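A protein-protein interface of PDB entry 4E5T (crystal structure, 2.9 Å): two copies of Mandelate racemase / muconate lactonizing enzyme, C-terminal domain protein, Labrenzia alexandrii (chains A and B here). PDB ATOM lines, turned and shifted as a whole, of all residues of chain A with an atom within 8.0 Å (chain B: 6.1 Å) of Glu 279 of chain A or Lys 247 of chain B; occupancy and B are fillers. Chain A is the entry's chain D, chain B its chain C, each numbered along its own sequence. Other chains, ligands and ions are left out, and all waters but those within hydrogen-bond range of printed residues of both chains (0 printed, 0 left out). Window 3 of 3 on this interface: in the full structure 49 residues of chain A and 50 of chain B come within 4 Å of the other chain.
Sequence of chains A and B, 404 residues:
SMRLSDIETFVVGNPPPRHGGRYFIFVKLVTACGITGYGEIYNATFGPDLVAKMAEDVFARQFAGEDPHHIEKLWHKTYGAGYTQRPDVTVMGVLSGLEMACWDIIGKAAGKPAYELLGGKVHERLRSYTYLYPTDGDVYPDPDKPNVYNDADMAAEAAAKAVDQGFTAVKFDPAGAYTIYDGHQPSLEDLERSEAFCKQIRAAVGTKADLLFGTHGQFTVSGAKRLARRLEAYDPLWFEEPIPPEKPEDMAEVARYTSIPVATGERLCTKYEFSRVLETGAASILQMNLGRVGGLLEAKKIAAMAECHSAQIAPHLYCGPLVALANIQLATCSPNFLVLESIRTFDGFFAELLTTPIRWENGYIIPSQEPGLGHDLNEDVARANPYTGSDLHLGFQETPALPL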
ATOM      1  N   GLN A  85      12.614  -1.409 -16.072  1.00  0.00           N
ATOM      2  CA  GLN A  85      12.761  -2.855 -15.953  1.00  0.00           C
ATOM      3  C   GLN A  85      13.393  -3.269 -14.617  1.00  0.00           C
ATOM      4  O   GLN A  85      14.385  -3.998 -14.575  1.00  0.00           O
ATOM      5  CB  GLN A  85      13.549  -3.396 -17.153  1.00  0.00           C
ATOM      6  CG  GLN A  85      13.422  -4.886 -17.384  1.00  0.00           C
ATOM      7  CD  GLN A  85      14.339  -5.363 -18.473  1.00  0.00           C
ATOM      8  OE1 GLN A  85      14.386  -4.772 -19.552  1.00  0.00           O
ATOM      9  NE2 GLN A  85      15.094  -6.424 -18.196  1.00  0.00           N
ATOM     10  N   ARG A  86      12.820  -2.754 -13.534  1.00  0.00           N
ATOM     11  CA  ARG A  86      13.156  -3.154 -12.167  1.00  0.00           C
ATOM     12  C   ARG A  86      11.949  -2.810 -11.311  1.00  0.00           C
ATOM     13  O   ARG A  86      11.252  -1.840 -11.585  1.00  0.00           O
ATOM     14  CB  ARG A  86      14.434  -2.473 -11.649  1.00  0.00           C
ATOM     15  CG  ARG A  86      14.690  -1.050 -12.150  1.00  0.00           C
ATOM     16  CD  ARG A  86      14.017   0.014 -11.292  1.00  0.00           C
ATOM     17  NE  ARG A  86      13.506  -0.516 -10.033  1.00  0.00           N
ATOM     18  CZ  ARG A  86      14.013  -0.223  -8.837  1.00  0.00           C
ATOM     19  NH1 ARG A  86      15.037   0.619  -8.726  1.00  0.00           N
ATOM     20  NH2 ARG A  86      13.501  -0.768  -7.746  1.00  0.00           N
ATOM     21  N   PRO A  87      11.669  -3.630 -10.300  1.00  0.00           N
ATOM     22  CA  PRO A  87      10.464  -3.468  -9.490  1.00  0.00           C
ATOM     23  C   PRO A  87      10.184  -2.025  -9.114  1.00  0.00           C
ATOM     24  O   PRO A  87      11.092  -1.229  -8.937  1.00  0.00           O
ATOM     25  CB  PRO A  87      10.788  -4.289  -8.252  1.00  0.00           C
ATOM     26  CG  PRO A  87      11.569  -5.423  -8.807  1.00  0.00           C
ATOM     27  CD  PRO A  87      12.435  -4.815  -9.893  1.00  0.00           C
ATOM     28  N   PRO A 248      16.121  -8.366   2.476  1.00  0.00           N
ATOM     29  CA  PRO A 248      15.644  -9.682   2.898  1.00  0.00           C
ATOM     30  C   PRO A 248      16.768 -10.496   3.512  1.00  0.00           C
ATOM     31  O   PRO A 248      16.507 -11.405   4.294  1.00  0.00           O
ATOM     32  CB  PRO A 248      15.178 -10.333   1.582  1.00  0.00           C
ATOM     33  CG  PRO A 248      15.035  -9.240   0.627  1.00  0.00           C
ATOM     34  CD  PRO A 248      16.064  -8.219   1.016  1.00  0.00           C
ATOM     35  N   ALA A 252      16.000 -12.672   6.924  1.00  0.00           N
ATOM     36  CA  ALA A 252      16.371 -14.057   7.081  1.00  0.00           C
ATOM     37  C   ALA A 252      17.076 -14.320   8.422  1.00  0.00           C
ATOM     38  O   ALA A 252      17.096 -15.441   8.906  1.00  0.00           O
ATOM     39  CB  ALA A 252      17.207 -14.508   5.898  1.00  0.00           C
ATOM     40  N   ARG A 256      15.759 -17.285  10.920  1.00  0.00           N
ATOM     41  CA  ARG A 256      16.637 -18.357  11.444  1.00  0.00           C
ATOM     42  C   ARG A 256      16.643 -18.471  12.975  1.00  0.00           C
ATOM     43  O   ARG A 256      16.711 -19.570  13.526  1.00  0.00           O
ATOM     44  CB  ARG A 256      18.086 -18.215  10.949  1.00  0.00           C
ATOM     45  CG  ARG A 256      18.350 -18.771   9.560  1.00  0.00           C
ATOM     46  CD  ARG A 256      19.836 -18.725   9.200  1.00  0.00           C
ATOM     47  NE  ARG A 256      20.364 -17.360   9.109  1.00  0.00           N
ATOM     48  CZ  ARG A 256      20.476 -16.671   7.975  1.00  0.00           C
ATOM     49  NH1 ARG A 256      20.094 -17.218   6.828  1.00  0.00           N
ATOM     50  NH2 ARG A 256      20.968 -15.437   7.984  1.00  0.00           N
ATOM     51  N   LYS A 271       8.368 -11.452  -9.673  1.00  0.00           N
ATOM     52  CA  LYS A 271       9.083 -12.682  -9.328  1.00  0.00           C
ATOM     53  C   LYS A 271      10.484 -12.399  -8.747  1.00  0.00           C
ATOM     54  O   LYS A 271      10.948 -13.113  -7.849  1.00  0.00           O
ATOM     55  CB  LYS A 271       9.193 -13.601 -10.557  1.00  0.00           C
ATOM     56  CG  LYS A 271       9.918 -12.944 -11.734  1.00  0.00           C
ATOM     57  CD  LYS A 271       9.915 -13.806 -12.965  1.00  0.00           C
ATOM     58  CE  LYS A 271       9.601 -12.974 -14.198  1.00  0.00           C
ATOM     59  NZ  LYS A 271       8.251 -12.348 -14.128  1.00  0.00           N
ATOM     60  N   TYR A 272      11.140 -11.356  -9.255  1.00  0.00           N
ATOM     61  CA  TYR A 272      12.497 -11.012  -8.823  1.00  0.00           C
ATOM     62  C   TYR A 272      12.628 -10.762  -7.317  1.00  0.00           C
ATOM     63  O   TYR A 272      13.570 -11.243  -6.683  1.00  0.00           O
ATOM     64  CB  TYR A 272      13.047  -9.838  -9.634  1.00  0.00           C
ATOM     65  CG  TYR A 272      12.947 -10.067 -11.128  1.00  0.00           C
ATOM     66  CD1 TYR A 272      13.679 -11.076 -11.746  1.00  0.00           C
ATOM     67  CD2 TYR A 272      12.111  -9.287 -11.919  1.00  0.00           C
ATOM     68  CE1 TYR A 272      13.583 -11.296 -13.102  1.00  0.00           C
ATOM     69  CE2 TYR A 272      12.021  -9.500 -13.270  1.00  0.00           C
ATOM     70  CZ  TYR A 272      12.759 -10.503 -13.854  1.00  0.00           C
ATOM     71  OH  TYR A 272      12.656 -10.722 -15.201  1.00  0.00           O
ATOM     72  N   GLU A 273      11.667 -10.050  -6.742  1.00  0.00           N
ATOM     73  CA  GLU A 273      11.713  -9.756  -5.317  1.00  0.00           C
ATOM     74  C   GLU A 273      11.313 -10.921  -4.411  1.00  0.00           C
ATOM     75  O   GLU A 273      11.731 -10.999  -3.259  1.00  0.00           O
ATOM     76  CB  GLU A 273      10.901  -8.503  -4.999  1.00  0.00           C
ATOM     77  CG  GLU A 273      11.677  -7.242  -5.290  1.00  0.00           C
ATOM     78  CD  GLU A 273      10.880  -5.985  -5.066  1.00  0.00           C
ATOM     79  OE1 GLU A 273       9.670  -6.087  -4.728  1.00  0.00           O
ATOM     80  OE2 GLU A 273      11.485  -4.896  -5.234  1.00  0.00           O
ATOM     81  N   PHE A 274      10.515 -11.838  -4.922  1.00  0.00           N
ATOM     82  CA  PHE A 274      10.195 -13.012  -4.129  1.00  0.00           C
ATOM     83  C   PHE A 274      11.250 -14.109  -4.288  1.00  0.00           C
ATOM     84  O   PHE A 274      11.474 -14.901  -3.377  1.00  0.00           O
ATOM     85  CB  PHE A 274       8.782 -13.505  -4.454  1.00  0.00           C
ATOM     86  CG  PHE A 274       7.716 -12.589  -3.963  1.00  0.00           C
ATOM     87  CD1 PHE A 274       7.338 -11.481  -4.704  1.00  0.00           C
ATOM     88  CD2 PHE A 274       7.120 -12.808  -2.738  1.00  0.00           C
ATOM     89  CE1 PHE A 274       6.359 -10.618  -4.237  1.00  0.00           C
ATOM     90  CE2 PHE A 274       6.145 -11.958  -2.271  1.00  0.00           C
ATOM     91  CZ  PHE A 274       5.763 -10.861  -3.022  1.00  0.00           C
ATOM     92  N   SER A 275      11.894 -14.152  -5.449  1.00  0.00           N
ATOM     93  CA  SER A 275      13.014 -15.050  -5.656  1.00  0.00           C
ATOM     94  C   SER A 275      14.048 -14.841  -4.547  1.00  0.00           C
ATOM     95  O   SER A 275      14.487 -15.803  -3.907  1.00  0.00           O
ATOM     96  CB  SER A 275      13.646 -14.791  -7.012  1.00  0.00           C
ATOM     97  OG  SER A 275      14.864 -15.502  -7.128  1.00  0.00           O
ATOM     98  N   ARG A 276      14.401 -13.578  -4.298  1.00  0.00           N
ATOM     99  CA  ARG A 276      15.351 -13.224  -3.239  1.00  0.00           C
ATOM    100  C   ARG A 276      14.867 -13.611  -1.838  1.00  0.00           C
ATOM    101  O   ARG A 276      15.629 -14.164  -1.058  1.00  0.00           O
ATOM    102  CB  ARG A 276      15.694 -11.730  -3.284  1.00  0.00           C
ATOM    103  CG  ARG A 276      16.576 -11.262  -2.116  1.00  0.00           C
ATOM    104  CD  ARG A 276      17.098  -9.843  -2.291  1.00  0.00           C
ATOM    105  NE  ARG A 276      17.851  -9.725  -3.536  1.00  0.00           N
ATOM    106  CZ  ARG A 276      17.402  -9.081  -4.608  1.00  0.00           C
ATOM    107  NH1 ARG A 276      16.219  -8.481  -4.563  1.00  0.00           N
ATOM    108  NH2 ARG A 276      18.133  -9.028  -5.714  1.00  0.00           N
ATOM    109  N   VAL A 277      13.608 -13.314  -1.519  1.00  0.00           N
ATOM    110  CA  VAL A 277      13.027 -13.704  -0.233  1.00  0.00           C
ATOM    111  C   VAL A 277      13.187 -15.195   0.041  1.00  0.00           C
ATOM    112  O   VAL A 277      13.660 -15.598   1.102  1.00  0.00           O
ATOM    113  CB  VAL A 277      11.522 -13.379  -0.139  1.00  0.00           C
ATOM    114  CG1 VAL A 277      10.923 -14.081   1.059  1.00  0.00           C
ATOM    115  CG2 VAL A 277      11.296 -11.884  -0.022  1.00  0.00           C
ATOM    116  N   LEU A 278      12.794 -16.010  -0.924  1.00  0.00           N
ATOM    117  CA  LEU A 278      12.895 -17.455  -0.796  1.00  0.00           C
ATOM    118  C   LEU A 278      14.335 -17.928  -0.647  1.00  0.00           C
ATOM    119  O   LEU A 278      14.660 -18.714   0.248  1.00  0.00           O
ATOM    120  CB  LEU A 278      12.277 -18.116  -2.023  1.00  0.00           C
ATOM    121  CG  LEU A 278      10.807 -17.805  -2.227  1.00  0.00           C
ATOM    122  CD1 LEU A 278      10.443 -18.204  -3.626  1.00  0.00           C
ATOM    123  CD2 LEU A 278       9.969 -18.534  -1.196  1.00  0.00           C
ATOM    124  N   GLU A 279      15.180 -17.443  -1.549  1.00  0.00           N
ATOM    125  CA  GLU A 279      16.571 -17.844  -1.605  1.00  0.00           C
ATOM    126  C   GLU A 279      17.342 -17.527  -0.328  1.00  0.00           C
ATOM    127  O   GLU A 279      18.114 -18.358   0.158  1.00  0.00           O
ATOM    128  CB  GLU A 279      17.236 -17.215  -2.819  1.00  0.00           C
ATOM    129  CG  GLU A 279      16.816 -17.877  -4.115  1.00  0.00           C
ATOM    130  CD  GLU A 279      17.358 -17.171  -5.339  1.00  0.00           C
ATOM    131  OE1 GLU A 279      18.045 -16.131  -5.188  1.00  0.00           O
ATOM    132  OE2 GLU A 279      17.082 -17.656  -6.456  1.00  0.00           O
ATOM    133  N   THR A 280      17.130 -16.344   0.230  1.00  0.00           N
ATOM    134  CA  THR A 280      17.841 -15.963   1.438  1.00  0.00           C
ATOM    135  C   THR A 280      17.252 -16.655   2.655  1.00  0.00           C
ATOM    136  O   THR A 280      17.911 -16.778   3.684  1.00  0.00           O
ATOM    137  CB  THR A 280      17.802 -14.455   1.671  1.00  0.00           C
ATOM    138  OG1 THR A 280      16.450 -14.045   1.905  1.00  0.00           O
ATOM    139  CG2 THR A 280      18.343 -13.724   0.467  1.00  0.00           C
ATOM    140  N   GLY A 281      16.010 -17.108   2.537  1.00  0.00           N
ATOM    141  CA  GLY A 281      15.301 -17.679   3.672  1.00  0.00           C
ATOM    142  C   GLY A 281      14.618 -16.607   4.498  1.00  0.00           C
ATOM    143  O   GLY A 281      14.330 -16.798   5.687  1.00  0.00           O
ATOM    144  N   ALA A 282      14.353 -15.475   3.853  1.00  0.00           N
ATOM    145  CA  ALA A 282      13.726 -14.326   4.490  1.00  0.00           C
ATOM    146  C   ALA A 282      12.366 -14.658   5.097  1.00  0.00           C
ATOM    147  O   ALA A 282      11.972 -14.070   6.098  1.00  0.00           O
ATOM    148  CB  ALA A 282      13.585 -13.188   3.480  1.00  0.00           C
ATOM    149  N   ALA A 283      11.654 -15.595   4.479  1.00  0.00           N
ATOM    150  CA  ALA A 283      10.287 -15.924   4.870  1.00  0.00           C
ATOM    151  C   ALA A 283       9.857 -17.272   4.271  1.00  0.00           C
ATOM    152  O   ALA A 283      10.466 -17.759   3.312  1.00  0.00           O
ATOM    153  CB  ALA A 283       9.331 -14.813   4.444  1.00  0.00           C
ATOM    154  N   MET A 305       7.706 -21.017  -7.384  1.00  0.00           N
ATOM    155  CA  MET A 305       9.041 -20.936  -6.808  1.00  0.00           C
ATOM    156  C   MET A 305       9.007 -21.384  -5.351  1.00  0.00           C
ATOM    157  O   MET A 305       9.829 -22.184  -4.918  1.00  0.00           O
ATOM    158  CB  MET A 305       9.596 -19.519  -6.928  1.00  0.00           C
ATOM    159  CG  MET A 305       9.794 -19.109  -8.370  1.00  0.00           C
ATOM    160  SD  MET A 305      10.682 -17.568  -8.618  1.00  0.00           S
ATOM    161  CE  MET A 305       9.403 -16.367  -8.288  1.00  0.00           C
ATOM    162  N   HIS A 309      11.129 -24.051  -2.370  1.00  0.00           N
ATOM    163  CA  HIS A 309      11.858 -23.552  -1.208  1.00  0.00           C
ATOM    164  C   HIS A 309      11.064 -23.718   0.081  1.00  0.00           C
ATOM    165  O   HIS A 309      11.271 -22.963   1.062  1.00  0.00           O
ATOM    166  CB  HIS A 309      12.286 -22.090  -1.389  1.00  0.00           C
ATOM    167  CG  HIS A 309      13.262 -21.883  -2.500  1.00  0.00           C
ATOM    168  ND1 HIS A 309      12.884 -21.420  -3.743  1.00  0.00           N
ATOM    169  CD2 HIS A 309      14.599 -22.086  -2.564  1.00  0.00           C
ATOM    170  CE1 HIS A 309      13.945 -21.342  -4.523  1.00  0.00           C
ATOM    171  NE2 HIS A 309      15.000 -21.735  -3.831  1.00  0.00           N
ATOM    172  N   ILE B 243      24.302  -6.843 -17.407  1.00  0.00           N
ATOM    173  CA  ILE B 243      23.069  -7.613 -17.279  1.00  0.00           C
ATOM    174  C   ILE B 243      21.976  -6.719 -16.668  1.00  0.00           C
ATOM    175  O   ILE B 243      22.261  -5.591 -16.264  1.00  0.00           O
ATOM    176  CB  ILE B 243      23.288  -8.894 -16.447  1.00  0.00           C
ATOM    177  CG1 ILE B 243      23.224  -8.588 -14.961  1.00  0.00           C
ATOM    178  CG2 ILE B 243      24.595  -9.554 -16.813  1.00  0.00           C
ATOM    179  CD1 ILE B 243      23.150  -9.816 -14.111  1.00  0.00           C
ATOM    180  N   PRO B 244      20.719  -7.193 -16.634  1.00  0.00           N
ATOM    181  CA  PRO B 244      19.625  -6.378 -16.076  1.00  0.00           C
ATOM    182  C   PRO B 244      19.712  -6.095 -14.563  1.00  0.00           C
ATOM    183  O   PRO B 244      20.447  -6.782 -13.855  1.00  0.00           O
ATOM    184  CB  PRO B 244      18.388  -7.211 -16.411  1.00  0.00           C
ATOM    185  CG  PRO B 244      18.769  -7.926 -17.660  1.00  0.00           C
ATOM    186  CD  PRO B 244      20.191  -8.319 -17.431  1.00  0.00           C
ATOM    187  N   PRO B 245      18.949  -5.099 -14.069  1.00  0.00           N
ATOM    188  CA  PRO B 245      19.181  -4.556 -12.725  1.00  0.00           C
ATOM    189  C   PRO B 245      18.701  -5.350 -11.515  1.00  0.00           C
ATOM    190  O   PRO B 245      19.125  -5.003 -10.416  1.00  0.00           O
ATOM    191  CB  PRO B 245      18.430  -3.212 -12.755  1.00  0.00           C
ATOM    192  CG  PRO B 245      18.200  -2.907 -14.200  1.00  0.00           C
ATOM    193  CD  PRO B 245      18.005  -4.255 -14.823  1.00  0.00           C
ATOM    194  N   GLU B 246      17.864  -6.368 -11.677  1.00  0.00           N
ATOM    195  CA  GLU B 246      17.118  -6.911 -10.524  1.00  0.00           C
ATOM    196  C   GLU B 246      17.889  -7.805  -9.527  1.00  0.00           C
ATOM    197  O   GLU B 246      17.558  -7.828  -8.338  1.00  0.00           O
ATOM    198  CB  GLU B 246      15.811  -7.585 -10.966  1.00  0.00           C
ATOM    199  CG  GLU B 246      15.021  -6.794 -11.999  1.00  0.00           C
ATOM    200  CD  GLU B 246      15.250  -7.318 -13.419  1.00  0.00           C
ATOM    201  OE1 GLU B 246      16.441  -7.608 -13.766  1.00  0.00           O
ATOM    202  OE2 GLU B 246      14.233  -7.462 -14.167  1.00  0.00           O
ATOM    203  N   LYS B 247      18.886  -8.547 -10.008  1.00  0.00           N
ATOM    204  CA  LYS B 247      19.753  -9.314  -9.122  1.00  0.00           C
ATOM    205  C   LYS B 247      21.195  -8.818  -9.242  1.00  0.00           C
ATOM    206  O   LYS B 247      21.906  -9.191 -10.170  1.00  0.00           O
ATOM    207  CB  LYS B 247      19.705 -10.820  -9.439  1.00  0.00           C
ATOM    208  CG  LYS B 247      18.341 -11.504  -9.359  1.00  0.00           C
ATOM    209  CD  LYS B 247      17.744 -11.488  -7.952  1.00  0.00           C
ATOM    210  CE  LYS B 247      16.900 -12.728  -7.702  1.00  0.00           C
ATOM    211  NZ  LYS B 247      17.744 -13.955  -7.570  1.00  0.00           N
ATOM    212  N   PRO B 248      21.642  -7.970  -8.303  1.00  0.00           N
ATOM    213  CA  PRO B 248      23.059  -7.594  -8.311  1.00  0.00           C
ATOM    214  C   PRO B 248      23.931  -8.805  -8.029  1.00  0.00           C
ATOM    215  O   PRO B 248      25.043  -8.888  -8.555  1.00  0.00           O
ATOM    216  CB  PRO B 248      23.163  -6.597  -7.155  1.00  0.00           C
ATOM    217  CG  PRO B 248      21.798  -6.069  -6.977  1.00  0.00           C
ATOM    218  CD  PRO B 248      20.890  -7.235  -7.277  1.00  0.00           C
ATOM    219  N   GLU B 249      23.407  -9.725  -7.220  1.00  0.00           N
ATOM    220  CA  GLU B 249      24.073 -10.983  -6.904  1.00  0.00           C
ATOM    221  C   GLU B 249      24.638 -11.656  -8.147  1.00  0.00           C
ATOM    222  O   GLU B 249      25.708 -12.265  -8.100  1.00  0.00           O
ATOM    223  CB  GLU B 249      23.101 -11.955  -6.218  1.00  0.00           C
ATOM    224  CG  GLU B 249      22.563 -11.526  -4.861  1.00  0.00           C
ATOM    225  CD  GLU B 249      21.214 -10.832  -4.955  1.00  0.00           C
ATOM    226  OE1 GLU B 249      20.872 -10.379  -6.072  1.00  0.00           O
ATOM    227  OE2 GLU B 249      20.501 -10.740  -3.921  1.00  0.00           O
ATOM    228  N   ASP B 250      23.905 -11.545  -9.255  1.00  0.00           N
ATOM    229  CA  ASP B 250      24.283 -12.189 -10.513  1.00  0.00           C
ATOM    230  C   ASP B 250      25.259 -11.346 -11.325  1.00  0.00           C
ATOM    231  O   ASP B 250      26.089 -11.878 -12.056  1.00  0.00           O
ATOM    232  CB  ASP B 250      23.047 -12.521 -11.361  1.00  0.00           C
ATOM    233  CG  ASP B 250      22.270 -13.733 -10.840  1.00  0.00           C
ATOM    234  OD1 ASP B 250      22.840 -14.554 -10.084  1.00  0.00           O
ATOM    235  OD2 ASP B 250      21.079 -13.865 -11.199  1.00  0.00           O
ATOM    236  N   MET B 251      25.163 -10.029 -11.194  1.00  0.00           N
ATOM    237  CA  MET B 251      26.086  -9.134 -11.882  1.00  0.00           C
ATOM    238  C   MET B 251      27.487  -9.343 -11.339  1.00  0.00           C
ATOM    239  O   MET B 251      28.468  -9.278 -12.081  1.00  0.00           O
ATOM    240  CB  MET B 251      25.664  -7.670 -11.710  1.00  0.00           C
ATOM    241  CG  MET B 251      26.587  -6.673 -12.405  1.00  0.00           C
ATOM    242  SD  MET B 251      26.000  -4.969 -12.300  1.00  0.00           S
ATOM    243  CE  MET B 251      24.743  -4.963 -13.590  1.00  0.00           C
ATOM    244  N   ALA B 252      27.576  -9.612 -10.041  1.00  0.00           N
ATOM    245  CA  ALA B 252      28.866  -9.788  -9.392  1.00  0.00           C
ATOM    246  C   ALA B 252      29.659 -10.981  -9.943  1.00  0.00           C
ATOM    247  O   ALA B 252      30.880 -11.046  -9.792  1.00  0.00           O
ATOM    248  CB  ALA B 252      28.683  -9.918  -7.916  1.00  0.00           C
ATOM    249  N   ARG B 276      23.379  -3.132  -1.772  1.00  0.00           N
ATOM    250  CA  ARG B 276      23.468  -4.494  -2.296  1.00  0.00           C
ATOM    251  C   ARG B 276      24.479  -4.608  -3.448  1.00  0.00           C
ATOM    252  O   ARG B 276      25.203  -5.603  -3.555  1.00  0.00           O
ATOM    253  CB  ARG B 276      22.082  -4.947  -2.720  1.00  0.00           C
ATOM    254  CG  ARG B 276      21.981  -6.281  -3.378  1.00  0.00           C
ATOM    255  CD  ARG B 276      20.503  -6.544  -3.677  1.00  0.00           C
ATOM    256  NE  ARG B 276      19.782  -6.975  -2.482  1.00  0.00           N
ATOM    257  CZ  ARG B 276      18.842  -6.274  -1.857  1.00  0.00           C
ATOM    258  NH1 ARG B 276      18.465  -5.085  -2.320  1.00  0.00           N
ATOM    259  NH2 ARG B 276      18.271  -6.779  -0.767  1.00  0.00           N
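The side-chain hydroxyl (OG) of Ser 275 of chain A is in hydrogen-bond range of the side-chain carboxylate (OE2) of Glu 279 of chain A (3.2 Å).
The backbone carbonyl oxygen (O) of Arg 276 of chain A is in hydrogen-bond range of the side-chain hydroxyl (OG1) of Thr 280 of chain A.
Among the printed residues, pairs that only touch across the chains: Gln 85 of chain A with Pro 244 of chain B, Gln 85 of chain A with Pro 245 of chain B, Pro 87 of chain A with Glu 246 of chain B, Pro 248 of chain A with Arg 276 of chain B, Tyr 272 of chain A with Glu 246 of chain B, Tyr 272 of chain A with Lys 247 of chain B, Arg 276 of chain A with Lys 247 of chain B, Arg 276 of chain A with Pro 248 of chain B and Arg 276 of chain A with Arg 276 of chain B.
Of the printed residues of chain B, Gln 85 of chain A touches Pro 244, Pro 245 and Glu 246.
Of the printed residues of chain B, Arg 276 of chain A touches Glu 246, Lys 247, Pro 248, Glu 249 and Arg 276.
Glu 279 of chain A touches one residue of chain B.
Thr 280 of chain A touches none of the printed residues of chain B.
Of the printed residues of chain A, Pro 244 of chain B touches Gln 85.
Printed residues of chain A within 4 Å of Glu 246 of chain B: Gln 85, Pro 87, Tyr 272 and Arg 276.
Of chain A, only Tyr 272 (3.8 Å), Ser 275 (3.3 Å), Arg 276 (3.3 Å) and Glu 279 (3.2 Å) come within 4 Å of Lys 247 of chain B.
Of chain A, only Arg 276 (3.6 Å) comes within 4 Å of Pro 248 of chain B.
The nearest printed residue of chain A that does not touch Lys 247 of chain B is Glu 273 of chain A (6.0 Å).
Of the 21 printed residues of chain A, 7 touch a printed residue of chain B.
Hydrophobic or aromatic side chains of chain A within 4 Å of the printed part of chain B: Pro 87, Pro 248 and Tyr 272.
Along chain A the printed residues that touch a printed residue of chain B span positions 85 to 279.
Printed residues of chain B that touch a printed residue of chain A: Pro 244, Pro 245, Glu 246, Lys 247, Pro 248, Glu 249 and Arg 276.
Hydrophobic or aromatic side chains of chain B that line the printed part of chain A: Pro 244, Pro 245 and Pro 248.
Among the printed residues, 14 pairs touch across the chains.
Pro 248 of chain A touches Arg 276 of chain B, and with the chains exchanged Arg 276 of chain A touches Pro 248 of chain B.
Arg 276 of chain B touches its own counterpart, Arg 276 of chain A.
Of the 14 pairs that touch across the chains among the printed residues, 3 have their exchanged pair printed and touching as well.
O of Glu 246 of chain B lies within hydrogen-bond range of NH2 of Arg 276 of chain A (2.9 Å).
NZ of Lys 247 of chain B is in hydrogen-bond range of OG of Ser 275 of chain A (3.3 Å).
The side-chain amino group (NZ) of Lys 247 of chain B lies within salt-bridge range of the side-chain carboxylate (OE1) of Glu 279 of chain A (3.2 Å).
The guanidinium group of Arg 276 of chain A is in salt-bridge range of the side-chain carboxylate of Glu 249 of chain B, at 2.9 Å.
O of Gln 85 of chain A lies close to OE2 of Glu 246 of chain B (3.5 Å).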
